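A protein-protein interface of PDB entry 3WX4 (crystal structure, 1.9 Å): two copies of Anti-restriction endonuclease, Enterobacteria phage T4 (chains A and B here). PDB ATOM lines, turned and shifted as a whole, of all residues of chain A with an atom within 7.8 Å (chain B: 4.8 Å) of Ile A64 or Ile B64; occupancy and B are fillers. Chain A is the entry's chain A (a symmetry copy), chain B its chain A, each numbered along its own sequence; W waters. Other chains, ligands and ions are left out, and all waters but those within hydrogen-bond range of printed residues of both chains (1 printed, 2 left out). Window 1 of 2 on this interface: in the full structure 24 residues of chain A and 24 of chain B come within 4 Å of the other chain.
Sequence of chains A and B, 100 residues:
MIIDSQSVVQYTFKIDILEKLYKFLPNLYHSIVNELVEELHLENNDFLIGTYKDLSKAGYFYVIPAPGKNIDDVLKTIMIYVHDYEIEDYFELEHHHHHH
Water W1 bridges O of Gln B10 and NE2 of Gln A6.
Printed residues of chain B that touch a printed residue of chain A: Val B8, Val B9, Gln B10, Phe B47, Leu B48, Tyr B62, Ile B64, Ala B66 and Pro B67. Hydrophobic or aromatic side chains of chain B that line the printed part of chain A: Val B8, Val B9, Leu B48, Tyr B62, Ile B64, Ala B66 and Pro B67. Along chain B the printed residues that touch a printed residue of chain A span positions 8 to 67. Hydrophobic or aromatic side chains of chain A that line the printed part of chain B: Val A8, Leu A48, Tyr A62, Ile A64, Ala A66 and Pro A67. Along chain A the printed residues that touch a printed residue of chain B span positions 6 to 67. Among the printed residues, 19 pairs touch across the chains.
Of the printed residues of chain B, Ile A64 touches Leu B48 (3.6 Å) and Ile B64 (3.9 Å). Ile B64 touches just these residues of chain A: Leu A48 (3.6 Å) and Ile A64 (3.9 Å). No residue of chain A comes within 4 Å of Pro B65. Printed residues of chain A within 4 Å of Ala B66: Leu A48 (3.8 Å) and Tyr A62 (3.8 Å). Of the printed residues of chain A, Phe B47 touches Leu A48 (3.9 Å). Ile A78 touches none of the printed residues of chain B. The nearest residue of chain B that does not touch Ile A64 is Pro B67 (4.2 Å). The nearest printed residue of chain B that does not touch Asn A45 is Tyr B62 (6.4 Å).
Val B9 touches Gln A6 (CA to O, 3.6 Å). Gln A10 touches Pro B67. Phe B47 touches Leu A48. Leu A48 touches Leu B48 (CG to CG, 3.5 Å). O of Ile B64 touches CD1 of Leu A48 (3.6 Å). Ala B66 touches Leu A48. Tyr A62 touches Pro B67 (CZ to CD, 3.3 Å). Ile A64 touches Ile B64 (CG2 to CG2, 3.9 Å). CA of Ala A66 touches CD1 of Leu B48, 3.8 Å away. Tyr B62 touches Ala A66.
O of Val B8 sits at hydrogen-bond distance from N of Val A8 (2.7 Å). The backbone NH (N) of Gln B10 lies within hydrogen-bond range of the backbone carbonyl oxygen (O) of Gln A6 (2.7 Å).
O of Asp B46 is in hydrogen-bond range of N of Ala B66 (2.8 Å). The backbone carbonyl oxygen (O) of Ile B64 lies within hydrogen-bond range of the backbone NH (N) of Leu B48, 2.8 Å away. N of Ala A66 lies within hydrogen-bond range of O of Asp A46, 2.8 Å away. O of Ile A64 sits at hydrogen-bond distance from N of Leu A48 (2.8 Å). The backbone carbonyl oxygen (O) of Gly A50 sits at hydrogen-bond distance from the backbone NH (N) of Tyr A62 (2.8 Å).
Gln A10 touches Pro B67, and with the chains exchanged Pro A67 touches Gln B10. Phe A47 touches Leu B48, and with the chains exchanged Leu A48 touches Phe B47. Leu A48 touches its own counterpart, Leu B48. Ile B64 touches its own counterpart, Ile A64. Of the 19 pairs that touch across the chains among the printed residues, 15 have their exchanged pair printed and touching as well.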
ATOM      1  N   GLN A   6     -19.778  18.848 -22.915  1.00  0.00           N
ATOM      2  CA  GLN A   6     -18.882  18.534 -24.011  1.00  0.00           C
ATOM      3  C   GLN A   6     -17.696  17.808 -23.398  1.00  0.00           C
ATOM      4  O   GLN A   6     -17.515  17.810 -22.182  1.00  0.00           O
ATOM      5  CB  GLN A   6     -18.441  19.806 -24.718  1.00  0.00           C
ATOM      6  CG  GLN A   6     -17.804  20.822 -23.808  1.00  0.00           C
ATOM      7  CD  GLN A   6     -17.443  22.099 -24.537  1.00  0.00           C
ATOM      8  OE1 GLN A   6     -16.556  22.106 -25.412  1.00  0.00           O
ATOM      9  NE2 GLN A   6     -18.127  23.202 -24.181  1.00  0.00           N
ATOM     10  N   VAL A   8     -13.746  17.027 -22.636  1.00  0.00           N
ATOM     11  CA  VAL A   8     -12.502  17.781 -22.460  1.00  0.00           C
ATOM     12  C   VAL A   8     -11.421  16.697 -22.235  1.00  0.00           C
ATOM     13  O   VAL A   8     -11.736  15.557 -21.932  1.00  0.00           O
ATOM     14  CB  VAL A   8     -12.644  18.772 -21.259  1.00  0.00           C
ATOM     15  CG1 VAL A   8     -13.094  18.038 -20.020  1.00  0.00           C
ATOM     16  CG2 VAL A   8     -11.350  19.521 -21.016  1.00  0.00           C
ATOM     17  N   VAL A   9     -10.155  17.030 -22.383  1.00  0.00           N
ATOM     18  CA  VAL A   9      -9.144  16.008 -22.216  1.00  0.00           C
ATOM     19  C   VAL A   9      -8.589  15.878 -20.804  1.00  0.00           C
ATOM     20  O   VAL A   9      -8.314  16.879 -20.152  1.00  0.00           O
ATOM     21  CB  VAL A   9      -7.974  16.270 -23.187  1.00  0.00           C
ATOM     22  CG1 VAL A   9      -6.933  15.151 -23.071  1.00  0.00           C
ATOM     23  CG2 VAL A   9      -8.528  16.332 -24.648  1.00  0.00           C
ATOM     24  N   GLN A  10      -8.434  14.644 -20.331  1.00  0.00           N
ATOM     25  CA  GLN A  10      -7.809  14.386 -19.018  1.00  0.00           C
ATOM     26  C   GLN A  10      -6.506  13.648 -19.379  1.00  0.00           C
ATOM     27  O   GLN A  10      -6.566  12.601 -20.022  1.00  0.00           O
ATOM     28  CB  GLN A  10      -8.684  13.475 -18.145  1.00  0.00           C
ATOM     29  CG  GLN A  10      -7.917  12.877 -16.946  1.00  0.00           C
ATOM     30  CD  GLN A  10      -8.801  12.031 -16.004  1.00  0.00           C
ATOM     31  OE1 GLN A  10      -8.381  10.955 -15.523  1.00  0.00           O
ATOM     32  NE2 GLN A  10     -10.002  12.521 -15.716  1.00  0.00           N
ATOM     33  N   TYR A  11      -5.341  14.170 -18.991  1.00  0.00           N
ATOM     34  CA  TYR A  11      -4.082  13.538 -19.349  1.00  0.00           C
ATOM     35  C   TYR A  11      -3.562  12.658 -18.215  1.00  0.00           C
ATOM     36  O   TYR A  11      -3.881  12.923 -17.059  1.00  0.00           O
ATOM     37  CB  TYR A  11      -3.013  14.602 -19.607  1.00  0.00           C
ATOM     38  CG  TYR A  11      -3.334  15.491 -20.770  1.00  0.00           C
ATOM     39  CD1 TYR A  11      -2.982  15.115 -22.055  1.00  0.00           C
ATOM     40  CD2 TYR A  11      -4.077  16.663 -20.603  1.00  0.00           C
ATOM     41  CE1 TYR A  11      -3.375  15.880 -23.171  1.00  0.00           C
ATOM     42  CE2 TYR A  11      -4.470  17.430 -21.716  1.00  0.00           C
ATOM     43  CZ  TYR A  11      -4.111  17.011 -22.994  1.00  0.00           C
ATOM     44  OH  TYR A  11      -4.548  17.684 -24.130  1.00  0.00           O
ATOM     45  N   THR A  12      -2.776  11.635 -18.566  1.00  0.00           N
ATOM     46  CA  THR A  12      -2.115  10.798 -17.572  1.00  0.00           C
ATOM     47  C   THR A  12      -0.660  11.186 -17.734  1.00  0.00           C
ATOM     48  O   THR A  12      -0.046  10.976 -18.795  1.00  0.00           O
ATOM     49  CB  THR A  12      -2.288   9.319 -17.850  1.00  0.00           C
ATOM     50  OG1 THR A  12      -3.648   8.981 -17.662  1.00  0.00           O
ATOM     51  CG2 THR A  12      -1.446   8.501 -16.896  1.00  0.00           C
ATOM     52  N   HIS A  41      -2.550  22.669  -6.121  1.00  0.00           N
ATOM     53  CA  HIS A  41      -3.901  23.196  -6.111  1.00  0.00           C
ATOM     54  C   HIS A  41      -3.988  24.537  -5.393  1.00  0.00           C
ATOM     55  O   HIS A  41      -4.785  25.398  -5.770  1.00  0.00           O
ATOM     56  CB  HIS A  41      -4.860  22.206  -5.449  1.00  0.00           C
ATOM     57  CG  HIS A  41      -5.239  21.076  -6.347  1.00  0.00           C
ATOM     58  ND1 HIS A  41      -5.607  19.833  -5.876  1.00  0.00           N
ATOM     59  CD2 HIS A  41      -5.319  21.012  -7.699  1.00  0.00           C
ATOM     60  CE1 HIS A  41      -5.903  19.052  -6.902  1.00  0.00           C
ATOM     61  NE2 HIS A  41      -5.739  19.744  -8.021  1.00  0.00           N
ATOM     62  N   ASN A  45      -4.658  27.955 -10.258  1.00  0.00           N
ATOM     63  CA  ASN A  45      -6.091  27.839 -10.394  1.00  0.00           C
ATOM     64  C   ASN A  45      -6.554  27.374 -11.733  1.00  0.00           C
ATOM     65  O   ASN A  45      -7.748  27.275 -11.930  1.00  0.00           O
ATOM     66  CB  ASN A  45      -6.746  29.190 -10.094  1.00  0.00           C
ATOM     67  CG  ASN A  45      -6.167  30.298 -10.966  1.00  0.00           C
ATOM     68  OD1 ASN A  45      -5.905  30.084 -12.182  1.00  0.00           O
ATOM     69  ND2 ASN A  45      -5.950  31.482 -10.369  1.00  0.00           N
ATOM     70  N   ASP A  46      -5.634  27.038 -12.627  1.00  0.00           N
ATOM     71  CA  ASP A  46      -5.980  26.634 -13.992  1.00  0.00           C
ATOM     72  C   ASP A  46      -5.816  25.154 -14.407  1.00  0.00           C
ATOM     73  O   ASP A  46      -5.743  24.820 -15.604  1.00  0.00           O
ATOM     74  CB  ASP A  46      -5.222  27.544 -14.991  1.00  0.00           C
ATOM     75  CG  ASP A  46      -3.722  27.671 -14.657  1.00  0.00           C
ATOM     76  OD1 ASP A  46      -3.237  26.932 -13.753  1.00  0.00           O
ATOM     77  OD2 ASP A  46      -3.018  28.501 -15.305  1.00  0.00           O
ATOM     78  N   PHE A  47      -5.750  24.245 -13.421  1.00  0.00           N
ATOM     79  CA  PHE A  47      -5.683  22.838 -13.776  1.00  0.00           C
ATOM     80  C   PHE A  47      -5.992  22.006 -12.530  1.00  0.00           C
ATOM     81  O   PHE A  47      -5.882  22.502 -11.410  1.00  0.00           O
ATOM     82  CB  PHE A  47      -4.318  22.439 -14.366  1.00  0.00           C
ATOM     83  CG  PHE A  47      -3.168  22.511 -13.406  1.00  0.00           C
ATOM     84  CD1 PHE A  47      -2.857  21.434 -12.557  1.00  0.00           C
ATOM     85  CD2 PHE A  47      -2.358  23.618 -13.379  1.00  0.00           C
ATOM     86  CE1 PHE A  47      -1.768  21.485 -11.718  1.00  0.00           C
ATOM     87  CE2 PHE A  47      -1.230  23.682 -12.520  1.00  0.00           C
ATOM     88  CZ  PHE A  47      -0.939  22.605 -11.681  1.00  0.00           C
ATOM     89  N   LEU A  48      -6.464  20.794 -12.764  1.00  0.00           N
ATOM     90  CA  LEU A  48      -6.757  19.852 -11.646  1.00  0.00           C
ATOM     91  C   LEU A  48      -5.689  18.785 -11.758  1.00  0.00           C
ATOM     92  O   LEU A  48      -5.219  18.465 -12.871  1.00  0.00           O
ATOM     93  CB  LEU A  48      -8.119  19.189 -11.842  1.00  0.00           C
ATOM     94  CG  LEU A  48      -9.349  20.069 -11.708  1.00  0.00           C
ATOM     95  CD1 LEU A  48     -10.588  19.250 -12.163  1.00  0.00           C
ATOM     96  CD2 LEU A  48      -9.505  20.539 -10.233  1.00  0.00           C
ATOM     97  N   ILE A  49      -5.279  18.207 -10.628  1.00  0.00           N
ATOM     98  CA  ILE A  49      -4.294  17.136 -10.698  1.00  0.00           C
ATOM     99  C   ILE A  49      -4.622  16.202  -9.543  1.00  0.00           C
ATOM    100  O   ILE A  49      -5.184  16.640  -8.515  1.00  0.00           O
ATOM    101  CB  ILE A  49      -2.869  17.659 -10.547  1.00  0.00           C
ATOM    102  CG1 ILE A  49      -1.888  16.502 -10.713  1.00  0.00           C
ATOM    103  CG2 ILE A  49      -2.709  18.401  -9.217  1.00  0.00           C
ATOM    104  CD1 ILE A  49      -0.444  16.924 -10.638  1.00  0.00           C
ATOM    105  N   GLY A  50      -4.313  14.923  -9.707  1.00  0.00           N
ATOM    106  CA  GLY A  50      -4.599  14.006  -8.608  1.00  0.00           C
ATOM    107  C   GLY A  50      -3.941  12.667  -8.895  1.00  0.00           C
ATOM    108  O   GLY A  50      -3.532  12.347 -10.029  1.00  0.00           O
ATOM    109  N   PHE A  61      -0.183  10.749 -12.582  1.00  0.00           N
ATOM    110  CA  PHE A  61      -1.174  11.750 -12.120  1.00  0.00           C
ATOM    111  C   PHE A  61      -2.170  12.044 -13.206  1.00  0.00           C
ATOM    112  O   PHE A  61      -1.784  12.012 -14.382  1.00  0.00           O
ATOM    113  CB  PHE A  61      -0.454  13.040 -11.758  1.00  0.00           C
ATOM    114  CG  PHE A  61       0.450  12.876 -10.604  1.00  0.00           C
ATOM    115  CD1 PHE A  61       0.001  13.178  -9.326  1.00  0.00           C
ATOM    116  CD2 PHE A  61       1.708  12.278 -10.770  1.00  0.00           C
ATOM    117  CE1 PHE A  61       0.787  12.880  -8.213  1.00  0.00           C
ATOM    118  CE2 PHE A  61       2.516  11.962  -9.672  1.00  0.00           C
ATOM    119  CZ  PHE A  61       2.045  12.263  -8.373  1.00  0.00           C
ATOM    120  N   TYR A  62      -3.434  12.276 -12.862  1.00  0.00           N
ATOM    121  CA  TYR A  62      -4.363  12.678 -13.921  1.00  0.00           C
ATOM    122  C   TYR A  62      -4.168  14.190 -13.949  1.00  0.00           C
ATOM    123  O   TYR A  62      -3.822  14.795 -12.915  1.00  0.00           O
ATOM    124  CB  TYR A  62      -5.827  12.303 -13.651  1.00  0.00           C
ATOM    125  CG  TYR A  62      -6.466  12.880 -12.391  1.00  0.00           C
ATOM    126  CD1 TYR A  62      -6.844  14.213 -12.334  1.00  0.00           C
ATOM    127  CD2 TYR A  62      -6.694  12.071 -11.265  1.00  0.00           C
ATOM    128  CE1 TYR A  62      -7.435  14.754 -11.196  1.00  0.00           C
ATOM    129  CE2 TYR A  62      -7.274  12.582 -10.102  1.00  0.00           C
ATOM    130  CZ  TYR A  62      -7.645  13.934 -10.071  1.00  0.00           C
ATOM    131  OH  TYR A  62      -8.196  14.531  -8.966  1.00  0.00           O
ATOM    132  N   VAL A  63      -4.332  14.805 -15.124  1.00  0.00           N
ATOM    133  CA  VAL A  63      -4.134  16.255 -15.234  1.00  0.00           C
ATOM    134  C   VAL A  63      -5.234  16.767 -16.174  1.00  0.00           C
ATOM    135  O   VAL A  63      -5.430  16.194 -17.259  1.00  0.00           O
ATOM    136  CB  VAL A  63      -2.759  16.585 -15.842  1.00  0.00           C
ATOM    137  CG1 VAL A  63      -2.601  18.078 -15.987  1.00  0.00           C
ATOM    138  CG2 VAL A  63      -1.650  16.091 -14.939  1.00  0.00           C
ATOM    139  N   ILE A  64      -5.994  17.756 -15.713  1.00  0.00           N
ATOM    140  CA  ILE A  64      -7.062  18.363 -16.492  1.00  0.00           C
ATOM    141  C   ILE A  64      -6.853  19.880 -16.475  1.00  0.00           C
ATOM    142  O   ILE A  64      -7.077  20.550 -15.455  1.00  0.00           O
ATOM    143  CB  ILE A  64      -8.456  18.044 -15.911  1.00  0.00           C
ATOM    144  CG1 ILE A  64      -8.644  16.529 -15.823  1.00  0.00           C
ATOM    145  CG2 ILE A  64      -9.583  18.574 -16.869  1.00  0.00           C
ATOM    146  CD1 ILE A  64      -9.780  16.112 -14.880  1.00  0.00           C
ATOM    147  N   PRO A  65      -6.398  20.440 -17.610  1.00  0.00           N
ATOM    148  CA  PRO A  65      -6.151  21.882 -17.749  1.00  0.00           C
ATOM    149  C   PRO A  65      -7.471  22.587 -17.980  1.00  0.00           C
ATOM    150  O   PRO A  65      -8.406  21.984 -18.540  1.00  0.00           O
ATOM    151  CB  PRO A  65      -5.225  21.948 -18.972  1.00  0.00           C
ATOM    152  CG  PRO A  65      -5.789  20.875 -19.840  1.00  0.00           C
ATOM    153  CD  PRO A  65      -6.029  19.721 -18.842  1.00  0.00           C
ATOM    154  N   ALA A  66      -7.578  23.829 -17.493  1.00  0.00           N
ATOM    155  CA  ALA A  66      -8.823  24.602 -17.681  1.00  0.00           C
ATOM    156  C   ALA A  66      -8.866  24.986 -19.168  1.00  0.00           C
ATOM    157  O   ALA A  66      -7.828  24.994 -19.815  1.00  0.00           O
ATOM    158  CB  ALA A  66      -8.805  25.885 -16.805  1.00  0.00           C
ATOM    159  N   PRO A  67     -10.056  25.301 -19.717  1.00  0.00           N
ATOM    160  CA  PRO A  67     -10.120  25.671 -21.141  1.00  0.00           C
ATOM    161  C   PRO A  67      -9.118  26.820 -21.389  1.00  0.00           C
ATOM    162  O   PRO A  67      -8.963  27.733 -20.559  1.00  0.00           O
ATOM    163  CB  PRO A  67     -11.588  26.098 -21.326  1.00  0.00           C
ATOM    164  CG  PRO A  67     -12.342  25.329 -20.230  1.00  0.00           C
ATOM    165  CD  PRO A  67     -11.369  25.466 -19.061  1.00  0.00           C
ATOM    166  N   LYS A  69      -5.913  26.614 -21.230  1.00  0.00           N
ATOM    167  CA  LYS A  69      -4.636  26.437 -20.562  1.00  0.00           C
ATOM    168  C   LYS A  69      -3.856  25.413 -21.373  1.00  0.00           C
ATOM    169  O   LYS A  69      -4.386  24.358 -21.751  1.00  0.00           O
ATOM    170  CB  LYS A  69      -4.796  25.936 -19.111  1.00  0.00           C
ATOM    171  CG  LYS A  69      -3.455  25.663 -18.416  1.00  0.00           C
ATOM    172  CD  LYS A  69      -2.633  26.932 -18.088  1.00  0.00           C
ATOM    173  CE  LYS A  69      -1.303  26.619 -17.414  1.00  0.00           C
ATOM    174  NZ  LYS A  69      -0.628  27.784 -16.717  1.00  0.00           N
ATOM    175  N   ILE A  71      -1.531  22.484 -21.894  1.00  0.00           N
ATOM    176  CA  ILE A  71      -1.100  21.336 -21.090  1.00  0.00           C
ATOM    177  C   ILE A  71       0.405  21.349 -20.858  1.00  0.00           C
ATOM    178  O   ILE A  71       0.858  21.136 -19.745  1.00  0.00           O
ATOM    179  CB  ILE A  71      -1.521  19.994 -21.736  1.00  0.00           C
ATOM    180  CG1 ILE A  71      -1.206  18.806 -20.794  1.00  0.00           C
ATOM    181  CG2 ILE A  71      -0.781  19.807 -23.022  1.00  0.00           C
ATOM    182  CD1 ILE A  71      -1.782  18.990 -19.403  1.00  0.00           C
ATOM    183  N   VAL A  74       1.391  23.317 -17.979  1.00  0.00           N
ATOM    184  CA  VAL A  74       1.018  22.677 -16.723  1.00  0.00           C
ATOM    185  C   VAL A  74       2.112  21.681 -16.328  1.00  0.00           C
ATOM    186  O   VAL A  74       2.521  21.637 -15.173  1.00  0.00           O
ATOM    187  CB  VAL A  74      -0.339  21.909 -16.818  1.00  0.00           C
ATOM    188  CG1 VAL A  74      -0.596  21.151 -15.472  1.00  0.00           C
ATOM    189  CG2 VAL A  74      -1.527  22.909 -17.102  1.00  0.00           C
ATOM    190  N   ILE A  78       4.293  21.509 -12.850  1.00  0.00           N
ATOM    191  CA  ILE A  78       4.324  20.317 -11.987  1.00  0.00           C
ATOM    192  C   ILE A  78       5.788  19.921 -11.735  1.00  0.00           C
ATOM    193  O   ILE A  78       6.202  19.730 -10.591  1.00  0.00           O
ATOM    194  CB  ILE A  78       3.561  19.155 -12.651  1.00  0.00           C
ATOM    195  CG1 ILE A  78       2.063  19.468 -12.710  1.00  0.00           C
ATOM    196  CG2 ILE A  78       3.799  17.816 -11.852  1.00  0.00           C
ATOM    197  CD1 ILE A  78       1.329  18.534 -13.629  1.00  0.00           C
ATOM    198  N   VAL B   8     -13.098  13.694 -20.627  1.00  0.00           N
ATOM    199  CA  VAL B   8     -13.789  13.919 -19.355  1.00  0.00           C
ATOM    200  C   VAL B   8     -14.917  14.922 -19.701  1.00  0.00           C
ATOM    201  O   VAL B   8     -14.881  15.565 -20.738  1.00  0.00           O
ATOM    202  CB  VAL B   8     -12.783  14.462 -18.289  1.00  0.00           C
ATOM    203  CG1 VAL B   8     -12.062  15.678 -18.816  1.00  0.00           C
ATOM    204  CG2 VAL B   8     -13.485  14.763 -16.981  1.00  0.00           C
ATOM    205  N   VAL B   9     -15.916  15.061 -18.853  1.00  0.00           N
ATOM    206  CA  VAL B   9     -16.992  15.967 -19.193  1.00  0.00           C
ATOM    207  C   VAL B   9     -16.818  17.393 -18.689  1.00  0.00           C
ATOM    208  O   VAL B   9     -16.410  17.602 -17.552  1.00  0.00           O
ATOM    209  CB  VAL B   9     -18.328  15.411 -18.656  1.00  0.00           C
ATOM    210  CG1 VAL B   9     -19.485  16.324 -19.075  1.00  0.00           C
ATOM    211  CG2 VAL B   9     -18.550  13.973 -19.228  1.00  0.00           C
ATOM    212  N   GLN B  10     -17.116  18.371 -19.540  1.00  0.00           N
ATOM    213  CA  GLN B  10     -17.086  19.791 -19.136  1.00  0.00           C
ATOM    214  C   GLN B  10     -18.562  20.223 -19.229  1.00  0.00           C
ATOM    215  O   GLN B  10     -19.156  20.110 -20.300  1.00  0.00           O
ATOM    216  CB  GLN B  10     -16.247  20.637 -20.106  1.00  0.00           C
ATOM    217  CG  GLN B  10     -16.498  22.152 -19.949  1.00  0.00           C
ATOM    218  CD  GLN B  10     -15.598  23.026 -20.851  1.00  0.00           C
ATOM    219  OE1 GLN B  10     -16.059  24.028 -21.441  1.00  0.00           O
ATOM    220  NE2 GLN B  10     -14.321  22.672 -20.937  1.00  0.00           N
ATOM    221  N   ASP B  46     -11.751  20.460  -5.842  1.00  0.00           N
ATOM    222  CA  ASP B  46     -12.246  19.370  -6.685  1.00  0.00           C
ATOM    223  C   ASP B  46     -13.055  19.707  -7.958  1.00  0.00           C
ATOM    224  O   ASP B  46     -13.792  18.863  -8.501  1.00  0.00           O
ATOM    225  CB  ASP B  46     -13.050  18.380  -5.803  1.00  0.00           C
ATOM    226  CG  ASP B  46     -14.077  19.091  -4.900  1.00  0.00           C
ATOM    227  OD1 ASP B  46     -14.283  20.327  -5.069  1.00  0.00           O
ATOM    228  OD2 ASP B  46     -14.695  18.414  -4.025  1.00  0.00           O
ATOM    229  N   PHE B  47     -12.933  20.951  -8.451  1.00  0.00           N
ATOM    230  CA  PHE B  47     -13.609  21.275  -9.694  1.00  0.00           C
ATOM    231  C   PHE B  47     -13.032  22.584 -10.235  1.00  0.00           C
ATOM    232  O   PHE B  47     -12.429  23.352  -9.487  1.00  0.00           O
ATOM    233  CB  PHE B  47     -15.136  21.388  -9.527  1.00  0.00           C
ATOM    234  CG  PHE B  47     -15.598  22.538  -8.682  1.00  0.00           C
ATOM    235  CD1 PHE B  47     -15.795  23.816  -9.233  1.00  0.00           C
ATOM    236  CD2 PHE B  47     -15.890  22.347  -7.355  1.00  0.00           C
ATOM    237  CE1 PHE B  47     -16.271  24.854  -8.465  1.00  0.00           C
ATOM    238  CE2 PHE B  47     -16.384  23.408  -6.552  1.00  0.00           C
ATOM    239  CZ  PHE B  47     -16.570  24.672  -7.115  1.00  0.00           C
ATOM    240  N   LEU B  48     -13.147  22.755 -11.541  1.00  0.00           N
ATOM    241  CA  LEU B  48     -12.678  24.008 -12.199  1.00  0.00           C
ATOM    242  C   LEU B  48     -13.949  24.715 -12.619  1.00  0.00           C
ATOM    243  O   LEU B  48     -14.967  24.064 -12.941  1.00  0.00           O
ATOM    244  CB  LEU B  48     -11.870  23.688 -13.455  1.00  0.00           C
ATOM    245  CG  LEU B  48     -10.517  23.028 -13.265  1.00  0.00           C
ATOM    246  CD1 LEU B  48      -9.983  22.596 -14.658  1.00  0.00           C
ATOM    247  CD2 LEU B  48      -9.536  24.021 -12.577  1.00  0.00           C
ATOM    248  N   TYR B  62     -18.416  27.301 -17.313  1.00  0.00           N
ATOM    249  CA  TYR B  62     -18.031  25.935 -17.677  1.00  0.00           C
ATOM    250  C   TYR B  62     -17.717  25.327 -16.315  1.00  0.00           C
ATOM    251  O   TYR B  62     -17.314  26.050 -15.384  1.00  0.00           O
ATOM    252  CB  TYR B  62     -16.825  25.852 -18.624  1.00  0.00           C
ATOM    253  CG  TYR B  62     -15.516  26.463 -18.130  1.00  0.00           C
ATOM    254  CD1 TYR B  62     -14.751  25.817 -17.170  1.00  0.00           C
ATOM    255  CD2 TYR B  62     -15.054  27.687 -18.643  1.00  0.00           C
ATOM    256  CE1 TYR B  62     -13.551  26.356 -16.713  1.00  0.00           C
ATOM    257  CE2 TYR B  62     -13.861  28.262 -18.199  1.00  0.00           C
ATOM    258  CZ  TYR B  62     -13.108  27.589 -17.227  1.00  0.00           C
ATOM    259  OH  TYR B  62     -11.939  28.088 -16.713  1.00  0.00           O
ATOM    260  N   VAL B  63     -17.944  24.018 -16.165  1.00  0.00           N
ATOM    261  CA  VAL B  63     -17.692  23.367 -14.874  1.00  0.00           C
ATOM    262  C   VAL B  63     -17.074  22.000 -15.198  1.00  0.00           C
ATOM    263  O   VAL B  63     -17.614  21.266 -16.043  1.00  0.00           O
ATOM    264  CB  VAL B  63     -18.999  23.155 -14.091  1.00  0.00           C
ATOM    265  CG1 VAL B  63     -18.717  22.443 -12.792  1.00  0.00           C
ATOM    266  CG2 VAL B  63     -19.636  24.486 -13.757  1.00  0.00           C
ATOM    267  N   ILE B  64     -15.914  21.719 -14.610  1.00  0.00           N
ATOM    268  CA  ILE B  64     -15.215  20.459 -14.799  1.00  0.00           C
ATOM    269  C   ILE B  64     -14.889  19.889 -13.415  1.00  0.00           C
ATOM    270  O   ILE B  64     -14.004  20.390 -12.704  1.00  0.00           O
ATOM    271  CB  ILE B  64     -13.900  20.636 -15.588  1.00  0.00           C
ATOM    272  CG1 ILE B  64     -14.192  21.300 -16.934  1.00  0.00           C
ATOM    273  CG2 ILE B  64     -13.263  19.237 -15.914  1.00  0.00           C
ATOM    274  CD1 ILE B  64     -12.948  21.909 -17.594  1.00  0.00           C
ATOM    275  N   PRO B  65     -15.621  18.838 -13.007  1.00  0.00           N
ATOM    276  CA  PRO B  65     -15.425  18.181 -11.706  1.00  0.00           C
ATOM    277  C   PRO B  65     -14.227  17.260 -11.798  1.00  0.00           C
ATOM    278  O   PRO B  65     -13.923  16.744 -12.889  1.00  0.00           O
ATOM    279  CB  PRO B  65     -16.744  17.419 -11.512  1.00  0.00           C
ATOM    280  CG  PRO B  65     -17.041  16.965 -12.902  1.00  0.00           C
ATOM    281  CD  PRO B  65     -16.741  18.225 -13.742  1.00  0.00           C
ATOM    282  N   ALA B  66     -13.508  17.103 -10.679  1.00  0.00           N
ATOM    283  CA  ALA B  66     -12.329  16.212 -10.666  1.00  0.00           C
ATOM    284  C   ALA B  66     -12.879  14.778 -10.729  1.00  0.00           C
ATOM    285  O   ALA B  66     -14.034  14.563 -10.389  1.00  0.00           O
ATOM    286  CB  ALA B  66     -11.515  16.408  -9.358  1.00  0.00           C
ATOM    287  N   PRO B  67     -12.065  13.798 -11.165  1.00  0.00           N
ATOM    288  CA  PRO B  67     -12.570  12.415 -11.236  1.00  0.00           C
ATOM    289  C   PRO B  67     -13.140  12.036  -9.851  1.00  0.00           C
ATOM    290  O   PRO B  67     -12.577  12.395  -8.801  1.00  0.00           O
ATOM    291  CB  PRO B  67     -11.320  11.604 -11.620  1.00  0.00           C
ATOM    292  CG  PRO B  67     -10.429  12.616 -12.357  1.00  0.00           C
ATOM    293  CD  PRO B  67     -10.625  13.857 -11.489  1.00  0.00           C
HETATM  294  O   HOH W   1     -20.297  22.168 -22.234  1.00  0.00           O
